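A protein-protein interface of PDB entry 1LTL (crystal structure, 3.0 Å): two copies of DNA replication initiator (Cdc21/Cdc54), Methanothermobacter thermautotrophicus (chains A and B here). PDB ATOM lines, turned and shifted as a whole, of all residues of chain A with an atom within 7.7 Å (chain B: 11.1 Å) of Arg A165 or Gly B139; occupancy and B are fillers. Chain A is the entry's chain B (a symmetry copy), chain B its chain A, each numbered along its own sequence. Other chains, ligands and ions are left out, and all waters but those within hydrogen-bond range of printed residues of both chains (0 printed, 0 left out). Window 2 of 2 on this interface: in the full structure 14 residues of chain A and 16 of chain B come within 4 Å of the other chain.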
ATOM      1  N   CYS A 137      -0.955   1.327 -16.623  1.00  0.00           N
ATOM      2  CA  CYS A 137      -1.154   1.779 -15.265  1.00  0.00           C
ATOM      3  C   CYS A 137      -2.360   2.726 -15.231  1.00  0.00           C
ATOM      4  O   CYS A 137      -2.384   3.737 -15.922  1.00  0.00           O
ATOM      5  CB  CYS A 137       0.072   2.515 -14.781  1.00  0.00           C
ATOM      6  SG  CYS A 137      -0.228   3.283 -13.203  1.00  0.00           S
ATOM      7  N   ARG A 138      -3.358   2.405 -14.420  1.00  0.00           N
ATOM      8  CA  ARG A 138      -4.540   3.235 -14.349  1.00  0.00           C
ATOM      9  C   ARG A 138      -4.290   4.567 -13.669  1.00  0.00           C
ATOM     10  O   ARG A 138      -5.144   5.451 -13.661  1.00  0.00           O
ATOM     11  CB  ARG A 138      -5.658   2.461 -13.661  1.00  0.00           C
ATOM     12  CG  ARG A 138      -6.028   1.247 -14.468  1.00  0.00           C
ATOM     13  CD  ARG A 138      -7.223   0.507 -13.941  1.00  0.00           C
ATOM     14  NE  ARG A 138      -8.100   0.139 -15.053  1.00  0.00           N
ATOM     15  CZ  ARG A 138      -8.869  -0.950 -15.083  1.00  0.00           C
ATOM     16  NH1 ARG A 138      -8.864  -1.795 -14.049  1.00  0.00           N
ATOM     17  NH2 ARG A 138      -9.653  -1.183 -16.138  1.00  0.00           N
ATOM     18  N   GLY A 139      -3.097   4.714 -13.113  1.00  0.00           N
ATOM     19  CA  GLY A 139      -2.745   5.938 -12.427  1.00  0.00           C
ATOM     20  C   GLY A 139      -2.211   7.001 -13.358  1.00  0.00           C
ATOM     21  O   GLY A 139      -2.652   8.134 -13.278  1.00  0.00           O
ATOM     22  N   GLU A 155      -0.072  -9.167 -12.166  1.00  0.00           N
ATOM     23  CA  GLU A 155       0.060  -7.717 -12.313  1.00  0.00           C
ATOM     24  C   GLU A 155       1.309  -7.203 -11.622  1.00  0.00           C
ATOM     25  O   GLU A 155       1.865  -7.866 -10.762  1.00  0.00           O
ATOM     26  CB  GLU A 155      -1.169  -6.999 -11.731  1.00  0.00           C
ATOM     27  CG  GLU A 155      -2.533  -7.586 -12.151  1.00  0.00           C
ATOM     28  CD  GLU A 155      -3.689  -6.586 -12.048  1.00  0.00           C
ATOM     29  OE1 GLU A 155      -3.703  -5.769 -11.087  1.00  0.00           O
ATOM     30  OE2 GLU A 155      -4.596  -6.627 -12.928  1.00  0.00           O
ATOM     31  N   PRO A 156       1.784  -6.022 -12.016  1.00  0.00           N
ATOM     32  CA  PRO A 156       2.973  -5.444 -11.401  1.00  0.00           C
ATOM     33  C   PRO A 156       2.713  -5.160  -9.921  1.00  0.00           C
ATOM     34  O   PRO A 156       1.569  -5.038  -9.497  1.00  0.00           O
ATOM     35  CB  PRO A 156       3.178  -4.174 -12.205  1.00  0.00           C
ATOM     36  CG  PRO A 156       2.709  -4.563 -13.534  1.00  0.00           C
ATOM     37  CD  PRO A 156       1.446  -5.305 -13.250  1.00  0.00           C
ATOM     38  N   SER A 157       3.773  -5.062  -9.132  1.00  0.00           N
ATOM     39  CA  SER A 157       3.629  -4.792  -7.701  1.00  0.00           C
ATOM     40  C   SER A 157       3.056  -3.390  -7.566  1.00  0.00           C
ATOM     41  O   SER A 157       1.986  -3.204  -6.997  1.00  0.00           O
ATOM     42  CB  SER A 157       4.994  -4.864  -7.010  1.00  0.00           C
ATOM     43  OG  SER A 157       5.632  -6.123  -7.229  1.00  0.00           O
ATOM     44  N   LEU A 158       3.784  -2.409  -8.084  1.00  0.00           N
ATOM     45  CA  LEU A 158       3.327  -1.044  -8.056  1.00  0.00           C
ATOM     46  C   LEU A 158       3.983  -0.317  -9.205  1.00  0.00           C
ATOM     47  O   LEU A 158       4.972  -0.789  -9.754  1.00  0.00           O
ATOM     48  CB  LEU A 158       3.694  -0.362  -6.745  1.00  0.00           C
ATOM     49  CG  LEU A 158       5.016   0.393  -6.693  1.00  0.00           C
ATOM     50  CD1 LEU A 158       5.104   1.255  -5.454  1.00  0.00           C
ATOM     51  CD2 LEU A 158       6.129  -0.602  -6.743  1.00  0.00           C
ATOM     52  N   CYS A 159       3.427   0.826  -9.583  1.00  0.00           N
ATOM     53  CA  CYS A 159       4.000   1.596 -10.666  1.00  0.00           C
ATOM     54  C   CYS A 159       5.061   2.496 -10.081  1.00  0.00           C
ATOM     55  O   CYS A 159       4.776   3.329  -9.236  1.00  0.00           O
ATOM     56  CB  CYS A 159       2.930   2.429 -11.346  1.00  0.00           C
ATOM     57  SG  CYS A 159       3.633   3.571 -12.517  1.00  0.00           S
ATOM     58  N   CYS A 162       4.483   6.620 -10.827  1.00  0.00           N
ATOM     59  CA  CYS A 162       3.520   7.418 -10.095  1.00  0.00           C
ATOM     60  C   CYS A 162       3.033   6.801  -8.787  1.00  0.00           C
ATOM     61  O   CYS A 162       2.281   7.432  -8.038  1.00  0.00           O
ATOM     62  CB  CYS A 162       2.316   7.711 -10.970  1.00  0.00           C
ATOM     63  SG  CYS A 162       1.234   6.318 -11.178  1.00  0.00           S
ATOM     64  N   GLY A 163       3.454   5.572  -8.510  1.00  0.00           N
ATOM     65  CA  GLY A 163       3.047   4.915  -7.282  1.00  0.00           C
ATOM     66  C   GLY A 163       1.731   4.170  -7.403  1.00  0.00           C
ATOM     67  O   GLY A 163       1.226   3.623  -6.426  1.00  0.00           O
ATOM     68  N   GLY A 164       1.173   4.134  -8.606  1.00  0.00           N
ATOM     69  CA  GLY A 164      -0.096   3.463  -8.786  1.00  0.00           C
ATOM     70  C   GLY A 164      -0.066   1.998  -8.412  1.00  0.00           C
ATOM     71  O   GLY A 164       0.987   1.371  -8.462  1.00  0.00           O
ATOM     72  N   ARG A 165      -1.212   1.442  -8.033  1.00  0.00           N
ATOM     73  CA  ARG A 165      -1.237   0.039  -7.701  1.00  0.00           C
ATOM     74  C   ARG A 165      -2.288  -0.696  -8.493  1.00  0.00           C
ATOM     75  O   ARG A 165      -2.498  -1.893  -8.311  1.00  0.00           O
ATOM     76  CB  ARG A 165      -1.467  -0.143  -6.213  1.00  0.00           C
ATOM     77  CG  ARG A 165      -0.215   0.059  -5.418  1.00  0.00           C
ATOM     78  CD  ARG A 165      -0.490  -0.145  -3.958  1.00  0.00           C
ATOM     79  NE  ARG A 165       0.705  -0.071  -3.125  1.00  0.00           N
ATOM     80  CZ  ARG A 165       1.457   1.014  -2.954  1.00  0.00           C
ATOM     81  NH1 ARG A 165       1.156   2.142  -3.560  1.00  0.00           N
ATOM     82  NH2 ARG A 165       2.512   0.983  -2.152  1.00  0.00           N
ATOM     83  N   SER A 166      -2.934   0.011  -9.405  1.00  0.00           N
ATOM     84  CA  SER A 166      -3.967  -0.610 -10.201  1.00  0.00           C
ATOM     85  C   SER A 166      -3.590  -0.633 -11.688  1.00  0.00           C
ATOM     86  O   SER A 166      -3.192   0.382 -12.242  1.00  0.00           O
ATOM     87  CB  SER A 166      -5.262   0.156  -9.949  1.00  0.00           C
ATOM     88  OG  SER A 166      -6.289  -0.257 -10.836  1.00  0.00           O
ATOM     89  N   PHE A 167      -3.717  -1.791 -12.327  1.00  0.00           N
ATOM     90  CA  PHE A 167      -3.363  -1.918 -13.729  1.00  0.00           C
ATOM     91  C   PHE A 167      -4.420  -2.597 -14.570  1.00  0.00           C
ATOM     92  O   PHE A 167      -5.241  -3.355 -14.064  1.00  0.00           O
ATOM     93  CB  PHE A 167      -2.063  -2.710 -13.884  1.00  0.00           C
ATOM     94  CG  PHE A 167      -0.926  -2.168 -13.096  1.00  0.00           C
ATOM     95  CD1 PHE A 167      -0.804  -2.445 -11.754  1.00  0.00           C
ATOM     96  CD2 PHE A 167      -0.016  -1.314 -13.683  1.00  0.00           C
ATOM     97  CE1 PHE A 167       0.207  -1.893 -11.017  1.00  0.00           C
ATOM     98  CE2 PHE A 167       1.002  -0.755 -12.941  1.00  0.00           C
ATOM     99  CZ  PHE A 167       1.101  -1.043 -11.611  1.00  0.00           C
ATOM    100  N   PHE B 135       4.509 -13.087   2.559  1.00  0.00           N
ATOM    101  CA  PHE B 135       3.646 -12.083   1.977  1.00  0.00           C
ATOM    102  C   PHE B 135       4.375 -10.786   1.688  1.00  0.00           C
ATOM    103  O   PHE B 135       5.359 -10.428   2.352  1.00  0.00           O
ATOM    104  CB  PHE B 135       2.474 -11.752   2.895  1.00  0.00           C
ATOM    105  CG  PHE B 135       1.601 -12.921   3.241  1.00  0.00           C
ATOM    106  CD1 PHE B 135       1.947 -13.780   4.263  1.00  0.00           C
ATOM    107  CD2 PHE B 135       0.405 -13.129   2.575  1.00  0.00           C
ATOM    108  CE1 PHE B 135       1.120 -14.824   4.608  1.00  0.00           C
ATOM    109  CE2 PHE B 135      -0.428 -14.173   2.919  1.00  0.00           C
ATOM    110  CZ  PHE B 135      -0.070 -15.017   3.934  1.00  0.00           C
ATOM    111  N   GLU B 136       3.876 -10.085   0.676  1.00  0.00           N
ATOM    112  CA  GLU B 136       4.406  -8.788   0.309  1.00  0.00           C
ATOM    113  C   GLU B 136       3.362  -7.797   0.806  1.00  0.00           C
ATOM    114  O   GLU B 136       2.186  -7.875   0.460  1.00  0.00           O
ATOM    115  CB  GLU B 136       4.532  -8.658  -1.197  1.00  0.00           C
ATOM    116  CG  GLU B 136       4.990  -7.291  -1.669  1.00  0.00           C
ATOM    117  CD  GLU B 136       4.773  -7.101  -3.170  1.00  0.00           C
ATOM    118  OE1 GLU B 136       3.609  -6.885  -3.605  1.00  0.00           O
ATOM    119  OE2 GLU B 136       5.775  -7.182  -3.923  1.00  0.00           O
ATOM    120  N   CYS B 137       3.793  -6.887   1.657  1.00  0.00           N
ATOM    121  CA  CYS B 137       2.902  -5.879   2.168  1.00  0.00           C
ATOM    122  C   CYS B 137       2.614  -4.874   1.048  1.00  0.00           C
ATOM    123  O   CYS B 137       3.528  -4.269   0.510  1.00  0.00           O
ATOM    124  CB  CYS B 137       3.545  -5.160   3.335  1.00  0.00           C
ATOM    125  SG  CYS B 137       2.537  -3.783   3.844  1.00  0.00           S
ATOM    126  N   ARG B 138       1.345  -4.689   0.708  1.00  0.00           N
ATOM    127  CA  ARG B 138       0.986  -3.772  -0.350  1.00  0.00           C
ATOM    128  C   ARG B 138       1.182  -2.329   0.029  1.00  0.00           C
ATOM    129  O   ARG B 138       1.046  -1.439  -0.795  1.00  0.00           O
ATOM    130  CB  ARG B 138      -0.448  -4.035  -0.789  1.00  0.00           C
ATOM    131  CG  ARG B 138      -0.575  -5.425  -1.348  1.00  0.00           C
ATOM    132  CD  ARG B 138      -1.925  -5.705  -1.937  1.00  0.00           C
ATOM    133  NE  ARG B 138      -1.772  -6.412  -3.204  1.00  0.00           N
ATOM    134  CZ  ARG B 138      -2.637  -7.305  -3.683  1.00  0.00           C
ATOM    135  NH1 ARG B 138      -3.737  -7.609  -2.987  1.00  0.00           N
ATOM    136  NH2 ARG B 138      -2.406  -7.889  -4.864  1.00  0.00           N
ATOM    137  N   GLY B 139       1.522  -2.100   1.283  1.00  0.00           N
ATOM    138  CA  GLY B 139       1.734  -0.750   1.750  1.00  0.00           C
ATOM    139  C   GLY B 139       3.143  -0.250   1.528  1.00  0.00           C
ATOM    140  O   GLY B 139       3.315   0.866   1.054  1.00  0.00           O
ATOM    141  N   CYS B 140       4.142  -1.067   1.862  1.00  0.00           N
ATOM    142  CA  CYS B 140       5.527  -0.678   1.724  1.00  0.00           C
ATOM    143  C   CYS B 140       6.337  -1.669   0.943  1.00  0.00           C
ATOM    144  O   CYS B 140       7.546  -1.570   0.864  1.00  0.00           O
ATOM    145  CB  CYS B 140       6.162  -0.496   3.087  1.00  0.00           C
ATOM    146  SG  CYS B 140       6.293  -2.018   4.007  1.00  0.00           S
ATOM    147  N   MET B 141       5.679  -2.652   0.371  1.00  0.00           N
ATOM    148  CA  MET B 141       6.388  -3.645  -0.429  1.00  0.00           C
ATOM    149  C   MET B 141       7.375  -4.521   0.336  1.00  0.00           C
ATOM    150  O   MET B 141       8.152  -5.214  -0.278  1.00  0.00           O
ATOM    151  CB  MET B 141       7.121  -2.956  -1.583  1.00  0.00           C
ATOM    152  CG  MET B 141       6.267  -2.010  -2.398  1.00  0.00           C
ATOM    153  SD  MET B 141       4.693  -2.728  -2.875  1.00  0.00           S
ATOM    154  CE  MET B 141       5.294  -4.122  -3.743  1.00  0.00           C
ATOM    155  N   ARG B 142       7.357  -4.497   1.663  1.00  0.00           N
ATOM    156  CA  ARG B 142       8.269  -5.342   2.432  1.00  0.00           C
ATOM    157  C   ARG B 142       7.770  -6.775   2.483  1.00  0.00           C
ATOM    158  O   ARG B 142       6.604  -7.028   2.216  1.00  0.00           O
ATOM    159  CB  ARG B 142       8.433  -4.814   3.845  1.00  0.00           C
ATOM    160  CG  ARG B 142       9.531  -3.803   3.968  1.00  0.00           C
ATOM    161  CD  ARG B 142       9.652  -3.324   5.394  1.00  0.00           C
ATOM    162  NE  ARG B 142       9.061  -2.009   5.517  1.00  0.00           N
ATOM    163  CZ  ARG B 142       9.760  -0.887   5.568  1.00  0.00           C
ATOM    164  NH1 ARG B 142      11.078  -0.921   5.529  1.00  0.00           N
ATOM    165  NH2 ARG B 142       9.131   0.270   5.606  1.00  0.00           N
ATOM    166  N   HIS B 143       8.647  -7.713   2.826  1.00  0.00           N
ATOM    167  CA  HIS B 143       8.260  -9.122   2.895  1.00  0.00           C
ATOM    168  C   HIS B 143       8.081  -9.621   4.334  1.00  0.00           C
ATOM    169  O   HIS B 143       8.864  -9.291   5.218  1.00  0.00           O
ATOM    170  CB  HIS B 143       9.298  -9.970   2.177  1.00  0.00           C
ATOM    171  CG  HIS B 143       9.246  -9.854   0.681  1.00  0.00           C
ATOM    172  ND1 HIS B 143       8.684  -8.775   0.032  1.00  0.00           N
ATOM    173  CD2 HIS B 143       9.673 -10.689  -0.300  1.00  0.00           C
ATOM    174  CE1 HIS B 143       8.759  -8.949  -1.275  1.00  0.00           C
ATOM    175  NE2 HIS B 143       9.354 -10.100  -1.504  1.00  0.00           N
ATOM    176  N   HIS B 144       7.029 -10.398   4.577  1.00  0.00           N
ATOM    177  CA  HIS B 144       6.749 -10.953   5.912  1.00  0.00           C
ATOM    178  C   HIS B 144       6.463 -12.444   5.750  1.00  0.00           C
ATOM    179  O   HIS B 144       5.721 -12.834   4.850  1.00  0.00           O
ATOM    180  CB  HIS B 144       5.503 -10.291   6.552  1.00  0.00           C
ATOM    181  CG  HIS B 144       5.662  -8.828   6.862  1.00  0.00           C
ATOM    182  ND1 HIS B 144       5.438  -7.832   5.931  1.00  0.00           N
ATOM    183  CD2 HIS B 144       6.021  -8.196   8.005  1.00  0.00           C
ATOM    184  CE1 HIS B 144       5.656  -6.657   6.486  1.00  0.00           C
ATOM    185  NE2 HIS B 144       6.010  -6.838   7.740  1.00  0.00           N
ATOM    186  N   GLU B 155      -3.302 -14.455   6.414  1.00  0.00           N
ATOM    187  CA  GLU B 155      -2.517 -13.241   6.220  1.00  0.00           C
ATOM    188  C   GLU B 155      -2.104 -12.642   7.548  1.00  0.00           C
ATOM    189  O   GLU B 155      -2.677 -12.947   8.580  1.00  0.00           O
ATOM    190  CB  GLU B 155      -3.315 -12.201   5.416  1.00  0.00           C
ATOM    191  CG  GLU B 155      -4.013 -12.741   4.152  1.00  0.00           C
ATOM    192  CD  GLU B 155      -4.308 -11.658   3.103  1.00  0.00           C
ATOM    193  OE1 GLU B 155      -4.652 -10.507   3.493  1.00  0.00           O
ATOM    194  OE2 GLU B 155      -4.206 -11.968   1.883  1.00  0.00           O
ATOM    195  N   PRO B 156      -1.070 -11.810   7.547  1.00  0.00           N
ATOM    196  CA  PRO B 156      -0.609 -11.174   8.780  1.00  0.00           C
ATOM    197  C   PRO B 156      -1.700 -10.250   9.328  1.00  0.00           C
ATOM    198  O   PRO B 156      -2.589  -9.821   8.590  1.00  0.00           O
ATOM    199  CB  PRO B 156       0.619 -10.402   8.319  1.00  0.00           C
ATOM    200  CG  PRO B 156       1.150 -11.256   7.251  1.00  0.00           C
ATOM    201  CD  PRO B 156      -0.078 -11.642   6.480  1.00  0.00           C
ATOM    202  N   LEU B 158      -1.267  -7.120  10.780  1.00  0.00           N
ATOM    203  CA  LEU B 158      -0.962  -5.835  10.215  1.00  0.00           C
ATOM    204  C   LEU B 158       0.538  -5.756  10.018  1.00  0.00           C
ATOM    205  O   LEU B 158       1.287  -6.517  10.613  1.00  0.00           O
ATOM    206  CB  LEU B 158      -1.414  -4.704  11.140  1.00  0.00           C
ATOM    207  CG  LEU B 158      -0.390  -4.167  12.143  1.00  0.00           C
ATOM    208  CD1 LEU B 158      -0.868  -2.886  12.771  1.00  0.00           C
ATOM    209  CD2 LEU B 158      -0.147  -5.215  13.164  1.00  0.00           C
ATOM    210  N   CYS B 159       0.975  -4.837   9.170  1.00  0.00           N
ATOM    211  CA  CYS B 159       2.387  -4.672   8.932  1.00  0.00           C
ATOM    212  C   CYS B 159       2.939  -3.746   9.988  1.00  0.00           C
ATOM    213  O   CYS B 159       2.534  -2.593  10.079  1.00  0.00           O
ATOM    214  CB  CYS B 159       2.635  -4.087   7.554  1.00  0.00           C
ATOM    215  SG  CYS B 159       4.364  -3.649   7.325  1.00  0.00           S
ATOM    216  N   SER B 160       3.875  -4.250  10.779  1.00  0.00           N
ATOM    217  CA  SER B 160       4.485  -3.466  11.857  1.00  0.00           C
ATOM    218  C   SER B 160       5.343  -2.299  11.395  1.00  0.00           C
ATOM    219  O   SER B 160       5.526  -1.334  12.134  1.00  0.00           O
ATOM    220  CB  SER B 160       5.335  -4.395  12.712  1.00  0.00           C
ATOM    221  OG  SER B 160       6.094  -5.252  11.867  1.00  0.00           O
ATOM    222  N   GLU B 161       5.856  -2.400  10.170  1.00  0.00           N
ATOM    223  CA  GLU B 161       6.730  -1.390   9.586  1.00  0.00           C
ATOM    224  C   GLU B 161       6.026  -0.145   9.115  1.00  0.00           C
ATOM    225  O   GLU B 161       6.526   0.954   9.321  1.00  0.00           O
ATOM    226  CB  GLU B 161       7.463  -1.984   8.404  1.00  0.00           C
ATOM    227  CG  GLU B 161       7.980  -3.366   8.668  1.00  0.00           C
ATOM    228  CD  GLU B 161       8.992  -3.358   9.769  1.00  0.00           C
ATOM    229  OE1 GLU B 161      10.017  -2.669   9.595  1.00  0.00           O
ATOM    230  OE2 GLU B 161       8.761  -4.030  10.799  1.00  0.00           O
ATOM    231  N   CYS B 162       4.880  -0.319   8.464  1.00  0.00           N
ATOM    232  CA  CYS B 162       4.147   0.822   7.958  1.00  0.00           C
ATOM    233  C   CYS B 162       2.681   0.895   8.366  1.00  0.00           C
ATOM    234  O   CYS B 162       1.990   1.865   8.043  1.00  0.00           O
ATOM    235  CB  CYS B 162       4.235   0.860   6.448  1.00  0.00           C
ATOM    236  SG  CYS B 162       3.181  -0.317   5.658  1.00  0.00           S
ATOM    237  N   GLY B 163       2.204  -0.122   9.072  1.00  0.00           N
ATOM    238  CA  GLY B 163       0.822  -0.133   9.508  1.00  0.00           C
ATOM    239  C   GLY B 163      -0.129  -0.689   8.467  1.00  0.00           C
ATOM    240  O   GLY B 163      -1.338  -0.696   8.652  1.00  0.00           O
ATOM    241  N   GLY B 164       0.409  -1.177   7.362  1.00  0.00           N
ATOM    242  CA  GLY B 164      -0.451  -1.701   6.319  1.00  0.00           C
ATOM    243  C   GLY B 164      -1.316  -2.855   6.769  1.00  0.00           C
ATOM    244  O   GLY B 164      -0.975  -3.551   7.709  1.00  0.00           O
ATOM    245  N   ARG B 165      -2.438  -3.067   6.103  1.00  0.00           N
ATOM    246  CA  ARG B 165      -3.279  -4.174   6.487  1.00  0.00           C
ATOM    247  C   ARG B 165      -3.601  -5.047   5.293  1.00  0.00           C
ATOM    248  O   ARG B 165      -4.354  -6.012   5.397  1.00  0.00           O
ATOM    249  CB  ARG B 165      -4.556  -3.663   7.141  1.00  0.00           C
ATOM    250  CG  ARG B 165      -4.356  -3.292   8.583  1.00  0.00           C
ATOM    251  CD  ARG B 165      -5.629  -2.804   9.169  1.00  0.00           C
ATOM    252  NE  ARG B 165      -5.530  -2.537  10.594  1.00  0.00           N
ATOM    253  CZ  ARG B 165      -4.798  -1.572  11.146  1.00  0.00           C
ATOM    254  NH1 ARG B 165      -4.079  -0.767  10.392  1.00  0.00           N
ATOM    255  NH2 ARG B 165      -4.815  -1.383  12.463  1.00  0.00           N
ATOM    256  N   SER B 166      -3.012  -4.729   4.154  1.00  0.00           N
ATOM    257  CA  SER B 166      -3.283  -5.498   2.962  1.00  0.00           C
ATOM    258  C   SER B 166      -2.017  -6.199   2.454  1.00  0.00           C
ATOM    259  O   SER B 166      -0.978  -5.574   2.305  1.00  0.00           O
ATOM    260  CB  SER B 166      -3.864  -4.550   1.920  1.00  0.00           C
ATOM    261  OG  SER B 166      -3.974  -5.185   0.659  1.00  0.00           O
ATOM    262  N   PHE B 167      -2.110  -7.498   2.197  1.00  0.00           N
ATOM    263  CA  PHE B 167      -0.964  -8.255   1.741  1.00  0.00           C
ATOM    264  C   PHE B 167      -1.224  -9.093   0.510  1.00  0.00           C
ATOM    265  O   PHE B 167      -2.364  -9.433   0.206  1.00  0.00           O
ATOM    266  CB  PHE B 167      -0.466  -9.180   2.843  1.00  0.00           C
ATOM    267  CG  PHE B 167      -0.175  -8.483   4.117  1.00  0.00           C
ATOM    268  CD1 PHE B 167      -1.190  -8.168   4.994  1.00  0.00           C
ATOM    269  CD2 PHE B 167       1.111  -8.090   4.421  1.00  0.00           C
ATOM    270  CE1 PHE B 167      -0.933  -7.466   6.137  1.00  0.00           C
ATOM    271  CE2 PHE B 167       1.371  -7.378   5.576  1.00  0.00           C
ATOM    272  CZ  PHE B 167       0.350  -7.071   6.432  1.00  0.00           C
ATOM    273  N   ARG B 168      -0.140  -9.427  -0.187  1.00  0.00           N
ATOM    274  CA  ARG B 168      -0.189 -10.252  -1.381  1.00  0.00           C
ATOM    275  C   ARG B 168       0.730 -11.438  -1.125  1.00  0.00           C
ATOM    276  O   ARG B 168       1.887 -11.268  -0.733  1.00  0.00           O
ATOM    277  CB  ARG B 168       0.311  -9.474  -2.594  1.00  0.00           C
ATOM    278  CG  ARG B 168       0.173 -10.232  -3.898  1.00  0.00           C
ATOM    279  CD  ARG B 168       1.412 -10.106  -4.764  1.00  0.00           C
ATOM    280  NE  ARG B 168       1.363  -8.925  -5.615  1.00  0.00           N
ATOM    281  CZ  ARG B 168       2.361  -8.528  -6.406  1.00  0.00           C
ATOM    282  NH1 ARG B 168       3.508  -9.213  -6.465  1.00  0.00           N
ATOM    283  NH2 ARG B 168       2.208  -7.439  -7.150  1.00  0.00           N
ATOM    284  N   LEU B 169       0.219 -12.641  -1.348  1.00  0.00           N
ATOM    285  CA  LEU B 169       1.008 -13.843  -1.113  1.00  0.00           C
ATOM    286  C   LEU B 169       2.002 -14.079  -2.214  1.00  0.00           C
ATOM    287  O   LEU B 169       1.643 -14.049  -3.375  1.00  0.00           O
ATOM    288  CB  LEU B 169       0.089 -15.051  -1.017  1.00  0.00           C
ATOM    289  CG  LEU B 169       0.759 -16.410  -0.941  1.00  0.00           C
ATOM    290  CD1 LEU B 169       1.652 -16.508   0.280  1.00  0.00           C
ATOM    291  CD2 LEU B 169      -0.304 -17.459  -0.895  1.00  0.00           C
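Among the printed residues, pairs that only touch across the chains: Glu A155 with Arg B168 (3.7 Å) and Ser A157 with Met B141 (3.4 Å).
Gly A139 touches none of the printed residues of chain B. Of the printed residues of chain B, Glu A155 touches Arg B168. Of the printed residues of chain B, Ser A157 touches Glu B136, Met B141 and Arg B168. No residue of chain B comes within 4 Å of Leu A158. No residue of chain B comes within 4 Å of Cys A159. No residue of chain B comes within 4 Å of Gly A164. Of chain B, only Arg B138 (2.7 Å) and Gly B139 (3.3 Å) come within 4 Å of Arg A165. No residue of chain B comes within 4 Å of Ser A166. Phe A167 touches none of the printed residues of chain B. Of chain A, only Arg A165 comes within 4 Å of Gly B139. Printed residues of chain A within 4 Å of Met B141: Ser A157. His B144 touches none of the printed residues of chain A. Of the printed residues of chain A, Arg B168 touches Glu A155, Pro A156 and Ser A157.
The side-chain carboxylate (OE1) of Glu B136 lies within salt-bridge range of the guanidinium group (NE) of Arg B168 (3.6 Å). SG of Cys B137 sits close to N of Gly B139 (3.2 Å). N of Arg B138 sits at hydrogen-bond distance from O of Ser B166 (3.0 Å). O of Gly A163 is in hydrogen-bond range of NH1 of Arg A165, 3.2 Å away.
Arg A165 touches Arg B138, but with the chains exchanged Arg A138 does not touch Arg B165 (20.3 Å). Arg A165 touches Gly B139, but with the chains exchanged Gly A139 does not touch Arg B165 (20.6 Å). Of the 7 pairs that touch across the chains among the printed residues, none has its exchanged pair printed and touching as well.
Of the 14 printed residues of chain A, 4 touch a printed residue of chain B. Among the printed residues, 7 pairs touch across the chains. Among the printed residues, no Asp or Glu carboxylate lies within 4 Å of a Lys or Arg side-chain nitrogen of the other chain.
The side-chain hydroxyl (OG) of Ser A157 sits at hydrogen-bond distance from the side-chain carboxylate (OE2) of Glu B136, 3.5 Å away. The guanidinium group (NE) of Arg A165 sits at hydrogen-bond distance from the backbone carbonyl oxygen (O) of Arg B138 (2.7 Å). NH2 of Arg A165 is in hydrogen-bond range of O of Gly B139 (3.3 Å). NH2 of Arg B168 sits at hydrogen-bond distance from O of Pro A156 (3.4 Å). The backbone NH (N) of Ser A157 sits close to the guanidinium group (NH2) of Arg B168, at 3.5 Å.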
